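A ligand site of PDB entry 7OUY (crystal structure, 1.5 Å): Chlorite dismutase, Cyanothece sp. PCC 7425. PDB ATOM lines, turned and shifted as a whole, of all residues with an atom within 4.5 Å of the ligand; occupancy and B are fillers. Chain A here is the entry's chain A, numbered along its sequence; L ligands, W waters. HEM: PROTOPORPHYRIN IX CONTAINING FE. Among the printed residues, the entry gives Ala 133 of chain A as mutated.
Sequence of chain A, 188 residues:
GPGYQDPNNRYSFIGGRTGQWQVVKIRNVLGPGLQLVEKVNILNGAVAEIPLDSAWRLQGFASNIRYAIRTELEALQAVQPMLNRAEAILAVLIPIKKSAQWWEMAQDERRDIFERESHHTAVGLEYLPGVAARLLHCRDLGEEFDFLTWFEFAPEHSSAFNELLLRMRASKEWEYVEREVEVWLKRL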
ATOM      1  N   ASN A  64      18.385   5.436  26.938  1.00  0.00           N
ATOM      2  CA  ASN A  64      18.114   4.079  26.538  1.00  0.00           C
ATOM      3  C   ASN A  64      16.617   3.850  26.391  1.00  0.00           C
ATOM      4  O   ASN A  64      15.788   4.608  26.912  1.00  0.00           O
ATOM      5  CB  ASN A  64      18.700   3.093  27.566  1.00  0.00           C
ATOM      6  CG  ASN A  64      18.098   3.273  28.948  1.00  0.00           C
ATOM      7  OD1 ASN A  64      18.492   4.170  29.691  1.00  0.00           O
ATOM      8  ND2 ASN A  64      17.117   2.465  29.279  1.00  0.00           N
ATOM      9  N   ILE A  65      16.289   2.761  25.714  1.00  0.00           N
ATOM     10  CA  ILE A  65      14.914   2.355  25.499  1.00  0.00           C
ATOM     11  C   ILE A  65      14.261   1.970  26.827  1.00  0.00           C
ATOM     12  O   ILE A  65      14.879   1.295  27.673  1.00  0.00           O
ATOM     13  CB  ILE A  65      14.849   1.187  24.485  1.00  0.00           C
ATOM     14  CG1 ILE A  65      15.194   1.709  23.072  1.00  0.00           C
ATOM     15  CG2 ILE A  65      13.496   0.515  24.533  1.00  0.00           C
ATOM     16  CD1 ILE A  65      14.168   2.663  22.481  1.00  0.00           C
ATOM     17  N   ARG A  66      13.024   2.413  27.012  1.00  0.00           N
ATOM     18  CA  ARG A  66      12.250   2.194  28.225  1.00  0.00           C
ATOM     19  C   ARG A  66      11.069   1.246  28.061  1.00  0.00           C
ATOM     20  O   ARG A  66      10.638   0.664  29.051  1.00  0.00           O
ATOM     21  CB  ARG A  66      11.712   3.538  28.751  1.00  0.00           C
ATOM     22  CG  ARG A  66      12.770   4.647  28.830  1.00  0.00           C
ATOM     23  CD  ARG A  66      13.998   4.244  29.636  1.00  0.00           C
ATOM     24  NE  ARG A  66      14.956   5.346  29.777  1.00  0.00           N
ATOM     25  CZ  ARG A  66      14.832   6.323  30.674  1.00  0.00           C
ATOM     26  NH1 ARG A  66      13.863   6.330  31.552  1.00  0.00           N
ATOM     27  NH2 ARG A  66      15.732   7.305  30.699  1.00  0.00           N
ATOM     28  N   TYR A  67      10.521   1.114  26.838  1.00  0.00           N
ATOM     29  CA  TYR A  67       9.339   0.312  26.625  1.00  0.00           C
ATOM     30  C   TYR A  67       9.416  -0.615  25.407  1.00  0.00           C
ATOM     31  O   TYR A  67       8.883  -1.732  25.441  1.00  0.00           O
ATOM     32  CB  TYR A  67       8.122   1.217  26.458  1.00  0.00           C
ATOM     33  CG  TYR A  67       7.821   2.022  27.690  1.00  0.00           C
ATOM     34  CD1 TYR A  67       7.305   1.415  28.832  1.00  0.00           C
ATOM     35  CD2 TYR A  67       8.056   3.393  27.734  1.00  0.00           C
ATOM     36  CE1 TYR A  67       7.023   2.144  29.961  1.00  0.00           C
ATOM     37  CE2 TYR A  67       7.771   4.135  28.865  1.00  0.00           C
ATOM     38  CZ  TYR A  67       7.264   3.489  29.991  1.00  0.00           C
ATOM     39  OH  TYR A  67       7.030   4.200  31.111  1.00  0.00           O
ATOM     40  N   ALA A  68      10.086  -0.178  24.352  1.00  0.00           N
ATOM     41  CA  ALA A  68      10.053  -0.925  23.093  1.00  0.00           C
ATOM     42  C   ALA A  68      10.797  -2.254  23.226  1.00  0.00           C
ATOM     43  O   ALA A  68      11.893  -2.320  23.781  1.00  0.00           O
ATOM     44  CB  ALA A  68      10.682  -0.094  21.976  1.00  0.00           C
ATOM     45  N   LEU A  76      11.192  -0.412  13.779  1.00  0.00           N
ATOM     46  CA  LEU A  76      11.502   1.020  13.768  1.00  0.00           C
ATOM     47  C   LEU A  76      12.780   1.296  13.000  1.00  0.00           C
ATOM     48  O   LEU A  76      12.823   2.194  12.141  1.00  0.00           O
ATOM     49  CB  LEU A  76      11.633   1.528  15.210  1.00  0.00           C
ATOM     50  CG  LEU A  76      10.334   1.600  16.011  1.00  0.00           C
ATOM     51  CD1 LEU A  76      10.610   1.453  17.503  1.00  0.00           C
ATOM     52  CD2 LEU A  76       9.624   2.913  15.726  1.00  0.00           C
ATOM     53  N   ILE A  94       7.831  19.315  20.609  1.00  0.00           N
ATOM     54  CA  ILE A  94       6.667  19.136  21.482  1.00  0.00           C
ATOM     55  C   ILE A  94       7.113  18.688  22.879  1.00  0.00           C
ATOM     56  O   ILE A  94       7.210  17.482  23.142  1.00  0.00           O
ATOM     57  CB  ILE A  94       5.685  18.124  20.877  1.00  0.00           C
ATOM     58  CG1 ILE A  94       5.296  18.550  19.461  1.00  0.00           C
ATOM     59  CG2 ILE A  94       4.452  17.967  21.748  1.00  0.00           C
ATOM     60  CD1 ILE A  94       4.235  17.675  18.810  1.00  0.00           C
ATOM     61  N   ILE A  96       6.508  17.630  26.654  1.00  0.00           N
ATOM     62  CA  ILE A  96       5.395  16.902  27.251  1.00  0.00           C
ATOM     63  C   ILE A  96       5.698  16.635  28.706  1.00  0.00           C
ATOM     64  O   ILE A  96       6.848  16.366  29.071  1.00  0.00           O
ATOM     65  CB  ILE A  96       5.127  15.580  26.502  1.00  0.00           C
ATOM     66  CG1 ILE A  96       4.656  15.881  25.069  1.00  0.00           C
ATOM     67  CG2 ILE A  96       4.126  14.743  27.263  1.00  0.00           C
ATOM     68  CD1 ILE A  96       4.369  14.660  24.253  1.00  0.00           C
ATOM     69  N   LYS A  98       3.935  14.295  31.981  1.00  0.00           N
ATOM     70  CA  LYS A  98       2.932  13.322  32.406  1.00  0.00           C
ATOM     71  C   LYS A  98       2.669  13.484  33.904  1.00  0.00           C
ATOM     72  O   LYS A  98       3.470  14.091  34.623  1.00  0.00           O
ATOM     73  CB  LYS A  98       3.397  11.896  32.095  1.00  0.00           C
ATOM     74  CG  LYS A  98       3.564  11.642  30.585  1.00  0.00           C
ATOM     75  CD  LYS A  98       3.776  10.178  30.267  1.00  0.00           C
ATOM     76  CE  LYS A  98       3.633   9.908  28.771  1.00  0.00           C
ATOM     77  NZ  LYS A  98       3.629   8.443  28.446  1.00  0.00           N
ATOM     78  N   TRP A 102       1.030   8.882  36.697  1.00  0.00           N
ATOM     79  CA  TRP A 102       1.728   8.069  35.699  1.00  0.00           C
ATOM     80  C   TRP A 102       3.044   7.538  36.259  1.00  0.00           C
ATOM     81  O   TRP A 102       3.336   6.348  36.184  1.00  0.00           O
ATOM     82  CB  TRP A 102       1.979   8.880  34.426  1.00  0.00           C
ATOM     83  CG  TRP A 102       2.911   8.185  33.456  1.00  0.00           C
ATOM     84  CD1 TRP A 102       4.232   8.413  33.304  1.00  0.00           C
ATOM     85  CD2 TRP A 102       2.563   7.166  32.514  1.00  0.00           C
ATOM     86  NE1 TRP A 102       4.745   7.592  32.341  1.00  0.00           N
ATOM     87  CE2 TRP A 102       3.737   6.810  31.831  1.00  0.00           C
ATOM     88  CE3 TRP A 102       1.363   6.524  32.174  1.00  0.00           C
ATOM     89  CZ2 TRP A 102       3.777   5.836  30.836  1.00  0.00           C
ATOM     90  CZ3 TRP A 102       1.387   5.561  31.179  1.00  0.00           C
ATOM     91  CH2 TRP A 102       2.576   5.227  30.521  1.00  0.00           C
ATOM     92  N   PHE A 114       1.073   1.942  27.379  1.00  0.00           N
ATOM     93  CA  PHE A 114       1.842   2.529  26.285  1.00  0.00           C
ATOM     94  C   PHE A 114       1.561   1.826  24.962  1.00  0.00           C
ATOM     95  O   PHE A 114       1.248   2.480  23.954  1.00  0.00           O
ATOM     96  CB  PHE A 114       3.342   2.484  26.621  1.00  0.00           C
ATOM     97  CG  PHE A 114       4.216   3.104  25.561  1.00  0.00           C
ATOM     98  CD1 PHE A 114       4.317   4.477  25.442  1.00  0.00           C
ATOM     99  CD2 PHE A 114       4.933   2.298  24.698  1.00  0.00           C
ATOM    100  CE1 PHE A 114       5.106   5.037  24.467  1.00  0.00           C
ATOM    101  CE2 PHE A 114       5.742   2.871  23.717  1.00  0.00           C
ATOM    102  CZ  PHE A 114       5.822   4.230  23.614  1.00  0.00           C
ATOM    103  N   HIS A 120       1.205   3.021  20.857  1.00  0.00           N
ATOM    104  CA  HIS A 120       2.041   4.173  20.508  1.00  0.00           C
ATOM    105  C   HIS A 120       3.008   3.828  19.393  1.00  0.00           C
ATOM    106  O   HIS A 120       3.134   4.564  18.403  1.00  0.00           O
ATOM    107  CB  HIS A 120       2.777   4.661  21.762  1.00  0.00           C
ATOM    108  CG  HIS A 120       3.584   5.908  21.578  1.00  0.00           C
ATOM    109  ND1 HIS A 120       3.359   7.048  22.311  1.00  0.00           N
ATOM    110  CD2 HIS A 120       4.619   6.200  20.753  1.00  0.00           C
ATOM    111  CE1 HIS A 120       4.210   7.988  21.939  1.00  0.00           C
ATOM    112  NE2 HIS A 120       5.004   7.501  21.001  1.00  0.00           N
ATOM    113  N   THR A 121       3.695   2.685  19.521  1.00  0.00           N
ATOM    114  CA  THR A 121       4.715   2.325  18.540  1.00  0.00           C
ATOM    115  C   THR A 121       4.090   1.898  17.223  1.00  0.00           C
ATOM    116  O   THR A 121       4.596   2.252  16.152  1.00  0.00           O
ATOM    117  CB  THR A 121       5.602   1.214  19.094  1.00  0.00           C
ATOM    118  OG1 THR A 121       6.053   1.577  20.397  1.00  0.00           O
ATOM    119  CG2 THR A 121       6.799   0.974  18.198  1.00  0.00           C
ATOM    120  N   GLY A 124       2.709   4.918  15.541  1.00  0.00           N
ATOM    121  CA  GLY A 124       3.839   5.703  15.086  1.00  0.00           C
ATOM    122  C   GLY A 124       4.462   5.169  13.812  1.00  0.00           C
ATOM    123  O   GLY A 124       4.825   5.934  12.916  1.00  0.00           O
ATOM    124  N   LEU A 125       4.619   3.848  13.736  1.00  0.00           N
ATOM    125  CA  LEU A 125       5.271   3.245  12.585  1.00  0.00           C
ATOM    126  C   LEU A 125       4.543   3.589  11.292  1.00  0.00           C
ATOM    127  O   LEU A 125       5.176   3.696  10.242  1.00  0.00           O
ATOM    128  CB  LEU A 125       5.339   1.726  12.745  1.00  0.00           C
ATOM    129  CG  LEU A 125       6.596   1.171  13.428  1.00  0.00           C
ATOM    130  CD1 LEU A 125       6.459  -0.317  13.689  1.00  0.00           C
ATOM    131  CD2 LEU A 125       7.839   1.452  12.578  1.00  0.00           C
ATOM    132  N   LEU A 128       6.062   6.731   9.658  1.00  0.00           N
ATOM    133  CA  LEU A 128       7.387   6.618   9.087  1.00  0.00           C
ATOM    134  C   LEU A 128       7.272   5.987   7.707  1.00  0.00           C
ATOM    135  O   LEU A 128       6.334   5.230   7.430  1.00  0.00           O
ATOM    136  CB  LEU A 128       8.273   5.766   9.977  1.00  0.00           C
ATOM    137  CG  LEU A 128       9.009   6.532  11.072  1.00  0.00           C
ATOM    138  CD1 LEU A 128       8.040   7.412  11.856  1.00  0.00           C
ATOM    139  CD2 LEU A 128       9.734   5.580  12.015  1.00  0.00           C
ATOM    140  N   VAL A 131       7.996  10.933   8.684  1.00  0.00           N
ATOM    141  CA  VAL A 131       8.282  11.721   9.879  1.00  0.00           C
ATOM    142  C   VAL A 131       9.491  11.129  10.603  1.00  0.00           C
ATOM    143  O   VAL A 131       9.480   9.955  10.994  1.00  0.00           O
ATOM    144  CB  VAL A 131       7.056  11.753  10.811  1.00  0.00           C
ATOM    145  CG1 VAL A 131       7.370  12.545  12.070  1.00  0.00           C
ATOM    146  CG2 VAL A 131       5.848  12.365  10.101  1.00  0.00           C
ATOM    147  N   ALA A 133      11.371  11.072  13.995  1.00  0.00           N
ATOM    148  CA  ALA A 133      10.971  11.286  15.389  1.00  0.00           C
ATOM    149  C   ALA A 133      12.137  10.984  16.318  1.00  0.00           C
ATOM    150  O   ALA A 133      12.802   9.965  16.159  1.00  0.00           O
ATOM    151  CB  ALA A 133       9.770  10.416  15.723  1.00  0.00           C
ATOM    152  N   LEU A 135      13.355  11.360  20.661  1.00  0.00           N
ATOM    153  CA  LEU A 135      12.868  11.516  22.028  1.00  0.00           C
ATOM    154  C   LEU A 135      14.009  11.865  22.957  1.00  0.00           C
ATOM    155  O   LEU A 135      15.059  11.205  22.946  1.00  0.00           O
ATOM    156  CB  LEU A 135      12.200  10.213  22.498  1.00  0.00           C
ATOM    157  CG  LEU A 135      11.806  10.160  23.982  1.00  0.00           C
ATOM    158  CD1 LEU A 135      10.665  11.181  24.245  1.00  0.00           C
ATOM    159  CD2 LEU A 135      11.335   8.779  24.324  1.00  0.00           C
ATOM    160  N   PHE A 147       9.431  15.223  28.832  1.00  0.00           N
ATOM    161  CA  PHE A 147      10.063  14.810  27.588  1.00  0.00           C
ATOM    162  C   PHE A 147      10.121  15.987  26.632  1.00  0.00           C
ATOM    163  O   PHE A 147       9.298  16.898  26.701  1.00  0.00           O
ATOM    164  CB  PHE A 147       9.314  13.665  26.889  1.00  0.00           C
ATOM    165  CG  PHE A 147       8.926  12.535  27.795  1.00  0.00           C
ATOM    166  CD1 PHE A 147       9.836  11.524  28.093  1.00  0.00           C
ATOM    167  CD2 PHE A 147       7.663  12.454  28.341  1.00  0.00           C
ATOM    168  CE1 PHE A 147       9.491  10.480  28.925  1.00  0.00           C
ATOM    169  CE2 PHE A 147       7.298  11.416  29.142  1.00  0.00           C
ATOM    170  CZ  PHE A 147       8.216  10.434  29.456  1.00  0.00           C
ATOM    171  N   THR A 149      10.091  16.038  22.585  1.00  0.00           N
ATOM    172  CA  THR A 149       9.957  15.209  21.396  1.00  0.00           C
ATOM    173  C   THR A 149      10.210  16.091  20.186  1.00  0.00           C
ATOM    174  O   THR A 149       9.771  17.244  20.151  1.00  0.00           O
ATOM    175  CB  THR A 149       8.585  14.549  21.333  1.00  0.00           C
ATOM    176  OG1 THR A 149       7.559  15.554  21.309  1.00  0.00           O
ATOM    177  CG2 THR A 149       8.394  13.650  22.546  1.00  0.00           C
ATOM    178  N   PHE A 151      10.383  16.316  15.827  1.00  0.00           N
ATOM    179  CA  PHE A 151       9.897  15.772  14.574  1.00  0.00           C
ATOM    180  C   PHE A 151      10.281  16.705  13.453  1.00  0.00           C
ATOM    181  O   PHE A 151      10.136  17.933  13.586  1.00  0.00           O
ATOM    182  CB  PHE A 151       8.366  15.576  14.603  1.00  0.00           C
ATOM    183  CG  PHE A 151       7.894  14.904  15.859  1.00  0.00           C
ATOM    184  CD1 PHE A 151       7.601  15.653  16.981  1.00  0.00           C
ATOM    185  CD2 PHE A 151       7.770  13.535  15.916  1.00  0.00           C
ATOM    186  CE1 PHE A 151       7.163  15.036  18.158  1.00  0.00           C
ATOM    187  CE2 PHE A 151       7.354  12.915  17.094  1.00  0.00           C
ATOM    188  CZ  PHE A 151       7.059  13.679  18.208  1.00  0.00           C
ATOM    189  N   PHE A 161       1.038  14.373   9.628  1.00  0.00           N
ATOM    190  CA  PHE A 161       1.515  14.609  10.983  1.00  0.00           C
ATOM    191  C   PHE A 161       0.380  15.127  11.869  1.00  0.00           C
ATOM    192  O   PHE A 161       0.191  14.671  13.000  1.00  0.00           O
ATOM    193  CB  PHE A 161       2.679  15.592  10.979  1.00  0.00           C
ATOM    194  CG  PHE A 161       3.361  15.723  12.304  1.00  0.00           C
ATOM    195  CD1 PHE A 161       4.095  14.673  12.826  1.00  0.00           C
ATOM    196  CD2 PHE A 161       3.267  16.897  13.042  1.00  0.00           C
ATOM    197  CE1 PHE A 161       4.726  14.785  14.052  1.00  0.00           C
ATOM    198  CE2 PHE A 161       3.890  17.015  14.269  1.00  0.00           C
ATOM    199  CZ  PHE A 161       4.629  15.954  14.769  1.00  0.00           C
ATOM    200  N   LEU A 164      -1.608  12.294  12.883  1.00  0.00           N
ATOM    201  CA  LEU A 164      -0.969  11.535  13.941  1.00  0.00           C
ATOM    202  C   LEU A 164      -1.197  12.191  15.297  1.00  0.00           C
ATOM    203  O   LEU A 164      -1.561  11.531  16.270  1.00  0.00           O
ATOM    204  CB  LEU A 164       0.513  11.395  13.632  1.00  0.00           C
ATOM    205  CG  LEU A 164       1.382  10.853  14.784  1.00  0.00           C
ATOM    206  CD1 LEU A 164       0.907   9.481  15.208  1.00  0.00           C
ATOM    207  CD2 LEU A 164       2.831  10.812  14.345  1.00  0.00           C
ATOM    208  N   LEU A 165      -0.963  13.505  15.383  1.00  0.00           N
ATOM    209  CA  LEU A 165      -1.151  14.189  16.655  1.00  0.00           C
ATOM    210  C   LEU A 165      -2.540  13.934  17.214  1.00  0.00           C
ATOM    211  O   LEU A 165      -2.710  13.777  18.425  1.00  0.00           O
ATOM    212  CB  LEU A 165      -0.910  15.686  16.496  1.00  0.00           C
ATOM    213  CG  LEU A 165       0.504  16.150  16.196  1.00  0.00           C
ATOM    214  CD1 LEU A 165       0.541  17.569  15.713  1.00  0.00           C
ATOM    215  CD2 LEU A 165       1.415  15.977  17.430  1.00  0.00           C
ATOM    216  N   MET A 168      -3.004  10.362  18.660  1.00  0.00           N
ATOM    217  CA  MET A 168      -2.288  10.165  19.925  1.00  0.00           C
ATOM    218  C   MET A 168      -2.935  10.939  21.063  1.00  0.00           C
ATOM    219  O   MET A 168      -3.106  10.404  22.163  1.00  0.00           O
ATOM    220  CB  MET A 168      -0.835  10.575  19.762  1.00  0.00           C
ATOM    221  CG  MET A 168      -0.178   9.927  18.574  1.00  0.00           C
ATOM    222  SD  MET A 168       1.544   9.640  18.778  1.00  0.00           S
ATOM    223  CE  MET A 168       1.566   7.836  18.879  1.00  0.00           C
ATOM    224  N   ARG A 169      -3.329  12.203  20.826  1.00  0.00           N
ATOM    225  CA  ARG A 169      -3.981  12.974  21.882  1.00  0.00           C
ATOM    226  C   ARG A 169      -5.313  12.357  22.296  1.00  0.00           C
ATOM    227  O   ARG A 169      -5.878  12.770  23.322  1.00  0.00           O
ATOM    228  CB  ARG A 169      -4.176  14.420  21.426  1.00  0.00           C
ATOM    229  CG  ARG A 169      -3.047  15.351  21.888  1.00  0.00           C
ATOM    230  CD  ARG A 169      -1.734  14.987  21.214  1.00  0.00           C
ATOM    231  NE  ARG A 169      -0.719  16.032  21.269  1.00  0.00           N
ATOM    232  CZ  ARG A 169      -0.768  17.182  20.605  1.00  0.00           C
ATOM    233  NH1 ARG A 169      -1.803  17.494  19.850  1.00  0.00           N
ATOM    234  NH2 ARG A 169       0.243  18.039  20.691  1.00  0.00           N
ATOM    235  N   GLU A 173      -3.006   6.608  26.686  1.00  0.00           N
ATOM    236  CA  GLU A 173      -1.746   7.137  27.197  1.00  0.00           C
ATOM    237  C   GLU A 173      -1.856   8.631  27.456  1.00  0.00           C
ATOM    238  O   GLU A 173      -1.288   9.147  28.417  1.00  0.00           O
ATOM    239  CB  GLU A 173      -0.600   6.840  26.216  1.00  0.00           C
ATOM    240  CG  GLU A 173       0.763   7.216  26.720  1.00  0.00           C
ATOM    241  CD  GLU A 173       1.800   7.394  25.623  1.00  0.00           C
ATOM    242  OE1 GLU A 173       1.511   7.017  24.453  1.00  0.00           O
ATOM    243  OE2 GLU A 173       2.934   7.865  25.941  1.00  0.00           O
ATOM    244  N   TRP A 174      -2.575   9.353  26.599  1.00  0.00           N
ATOM    245  CA  TRP A 174      -2.634  10.802  26.733  1.00  0.00           C
ATOM    246  C   TRP A 174      -3.551  11.259  27.860  1.00  0.00           C
ATOM    247  O   TRP A 174      -3.580  12.456  28.170  1.00  0.00           O
ATOM    248  CB  TRP A 174      -3.060  11.441  25.409  1.00  0.00           C
ATOM    249  CG  TRP A 174      -1.955  12.264  24.847  1.00  0.00           C
ATOM    250  CD1 TRP A 174      -1.865  13.617  24.856  1.00  0.00           C
ATOM    251  CD2 TRP A 174      -0.770  11.778  24.225  1.00  0.00           C
ATOM    252  NE1 TRP A 174      -0.696  14.013  24.271  1.00  0.00           N
ATOM    253  CE2 TRP A 174       0.007  12.895  23.886  1.00  0.00           C
ATOM    254  CE3 TRP A 174      -0.277  10.501  23.929  1.00  0.00           C
ATOM    255  CZ2 TRP A 174       1.245  12.779  23.256  1.00  0.00           C
ATOM    256  CZ3 TRP A 174       0.943  10.395  23.309  1.00  0.00           C
ATOM    257  CH2 TRP A 174       1.694  11.526  22.981  1.00  0.00           C
ATOM    258  N   GLU A 180       1.484  20.222  27.659  1.00  0.00           N
ATOM    259  CA  GLU A 180       1.917  19.966  26.302  1.00  0.00           C
ATOM    260  C   GLU A 180       1.899  21.258  25.500  1.00  0.00           C
ATOM    261  O   GLU A 180       0.945  22.043  25.599  1.00  0.00           O
ATOM    262  CB  GLU A 180       1.023  18.909  25.635  1.00  0.00           C
ATOM    263  CG  GLU A 180       1.499  18.428  24.287  1.00  0.00           C
ATOM    264  CD  GLU A 180       0.730  17.226  23.800  1.00  0.00           C
ATOM    265  OE1 GLU A 180      -0.341  16.925  24.377  1.00  0.00           O
ATOM    266  OE2 GLU A 180       1.204  16.564  22.849  1.00  0.00           O
HETATM  267  CHA HEM L   1       8.170   7.385  23.228  1.00  0.00           C
HETATM  268  CHB HEM L   1       7.738   5.866  18.645  1.00  0.00           C
HETATM  269  CHC HEM L   1       5.400   9.974  17.536  1.00  0.00           C
HETATM  270  CHD HEM L   1       5.644  11.405  22.151  1.00  0.00           C
HETATM  271  C1A HEM L   1       8.220   6.575  22.118  1.00  0.00           C
HETATM  272  C2A HEM L   1       8.657   5.207  22.027  1.00  0.00           C
HETATM  273  C3A HEM L   1       8.535   4.797  20.774  1.00  0.00           C
HETATM  274  C4A HEM L   1       7.994   5.895  20.001  1.00  0.00           C
HETATM  275  CMA HEM L   1       8.878   3.394  20.222  1.00  0.00           C
HETATM  276  CAA HEM L   1       9.192   4.323  23.189  1.00  0.00           C
HETATM  277  CBA HEM L   1      10.646   4.682  23.434  1.00  0.00           C
HETATM  278  CGA HEM L   1      11.204   3.815  24.559  1.00  0.00           C
HETATM  279  O1A HEM L   1      11.898   4.381  25.406  1.00  0.00           O
HETATM  280  O2A HEM L   1      10.897   2.605  24.556  1.00  0.00           O
HETATM  281  C1B HEM L   1       7.127   6.874  17.933  1.00  0.00           C
HETATM  282  C2B HEM L   1       7.028   6.941  16.494  1.00  0.00           C
HETATM  283  C3B HEM L   1       6.415   8.075  16.178  1.00  0.00           C
HETATM  284  C4B HEM L   1       6.064   8.770  17.388  1.00  0.00           C
HETATM  285  CMB HEM L   1       7.573   5.897  15.508  1.00  0.00           C
HETATM  286  CAB HEM L   1       6.094   8.533  14.742  1.00  0.00           C
HETATM  287  CBB HEM L   1       5.923   9.827  14.467  1.00  0.00           C
HETATM  288  C1C HEM L   1       5.209  10.713  18.674  1.00  0.00           C
HETATM  289  C2C HEM L   1       4.475  11.938  18.821  1.00  0.00           C
HETATM  290  C3C HEM L   1       4.545  12.340  20.099  1.00  0.00           C
HETATM  291  C4C HEM L   1       5.339  11.356  20.809  1.00  0.00           C
HETATM  292  CMC HEM L   1       3.742  12.649  17.656  1.00  0.00           C
HETATM  293  CAC HEM L   1       3.925  13.573  20.773  1.00  0.00           C
HETATM  294  CBC HEM L   1       2.883  14.229  20.256  1.00  0.00           C
HETATM  295  C1D HEM L   1       6.372  10.431  22.847  1.00  0.00           C
HETATM  296  C2D HEM L   1       6.644  10.463  24.255  1.00  0.00           C
HETATM  297  C3D HEM L   1       7.346   9.373  24.545  1.00  0.00           C
HETATM  298  C4D HEM L   1       7.525   8.582  23.346  1.00  0.00           C
HETATM  299  CMD HEM L   1       6.220  11.583  25.192  1.00  0.00           C
HETATM  300  CAD HEM L   1       7.875   8.978  25.956  1.00  0.00           C
HETATM  301  CBD HEM L   1       6.879   8.008  26.575  1.00  0.00           C
HETATM  302  CGD HEM L   1       7.280   7.638  27.981  1.00  0.00           C
HETATM  303  O1D HEM L   1       6.404   7.638  28.886  1.00  0.00           O
HETATM  304  O2D HEM L   1       8.496   7.364  28.218  1.00  0.00           O
HETATM  305  NA  HEM L   1       7.822   6.964  20.848  1.00  0.00           N
HETATM  306  NB  HEM L   1       6.551   8.015  18.444  1.00  0.00           N
HETATM  307  NC  HEM L   1       5.716  10.381  19.912  1.00  0.00           N
HETATM  308  ND  HEM L   1       6.890   9.274  22.308  1.00  0.00           N
HETATM  309 FE   HEM L   1       6.587   8.596  20.419  1.00  0.00          FE
HETATM  310  O   HOH W   1      10.515   6.379  26.649  1.00  0.00           O
HETATM  311  O   HOH W   2       9.897   6.856  30.586  1.00  0.00           O
HETATM  312  O   HOH W   3       7.205   6.736  31.082  1.00  0.00           O
HETATM  313  O   HOH W   4      13.983   6.126  25.363  1.00  0.00           O
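A ring nitrogen (NE2) of His 120 is bound to an iron atom (FE) of the ligand, 2.0 Å away.
N of Tyr 67 lies within hydrogen-bond range of O2A of the ligand, at 2.8 Å.
An oxygen (O1A) of the ligand sits at hydrogen-bond distance from the backbone NH (N) of Arg 66, at 2.8 Å.
The backbone NH (N) of Ala 68 is in hydrogen-bond range of an oxygen (O2A) of the ligand, 2.9 Å away.
The side-chain amino group (NZ) of Lys 98 lies within salt-bridge range of an oxygen (O1D) of the ligand.
The backbone NH (N) of His 120 sits at hydrogen-bond distance from the backbone carbonyl oxygen (O) of Phe 114 (3.1 Å).
ND1 of His 120 sits at hydrogen-bond distance from OE1 of Glu 173, at 2.8 Å.
The backbone carbonyl oxygen of Asn 64 is in hydrogen-bond range of the guanidinium group of Arg 66 (3.1 Å).
The side-chain carboxylate (OE2) of Glu 173 is in salt-bridge range of the side-chain amino group (NZ) of Lys 98 (2.7 Å).
The backbone NH of Phe 147 lies within hydrogen-bond range of the backbone carbonyl oxygen of Ile 96.
The side-chain hydroxyl (OG1) of Thr 149 sits at hydrogen-bond distance from the backbone carbonyl oxygen (O) of Ile 94.
The side-chain carboxylate (OE1) of Glu 180 is in hydrogen-bond range of the indole nitrogen (NE1) of Trp 174.
The side-chain carboxylate (OE2) of Glu 180 is in salt-bridge range of the guanidinium group (NE) of Arg 169, 2.5 Å away.
Residues that only touch the ligand: Phe 151, Leu 164, Phe 147, Ile 65, Thr 121, Phe 114, Gly 124, Thr 149, Leu 76, Leu 135, Leu 165, Leu 128, Ile 96, Trp 174, Met 168, Trp 102, Glu 180, Val 131, Ile 94 and Glu 173.
Of the 30 residues printed, 25 come within 4 Å of the ligand.
Water W3 lies within hydrogen-bond range of O1D of the ligand (2.5 Å), OH of Tyr 67 (2.5 Å) and NE1 of Trp 102 (2.9 Å).
Water W4 lies within hydrogen-bond range of O1A of the ligand (2.7 Å) and O of Asn 64 (2.8 Å).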
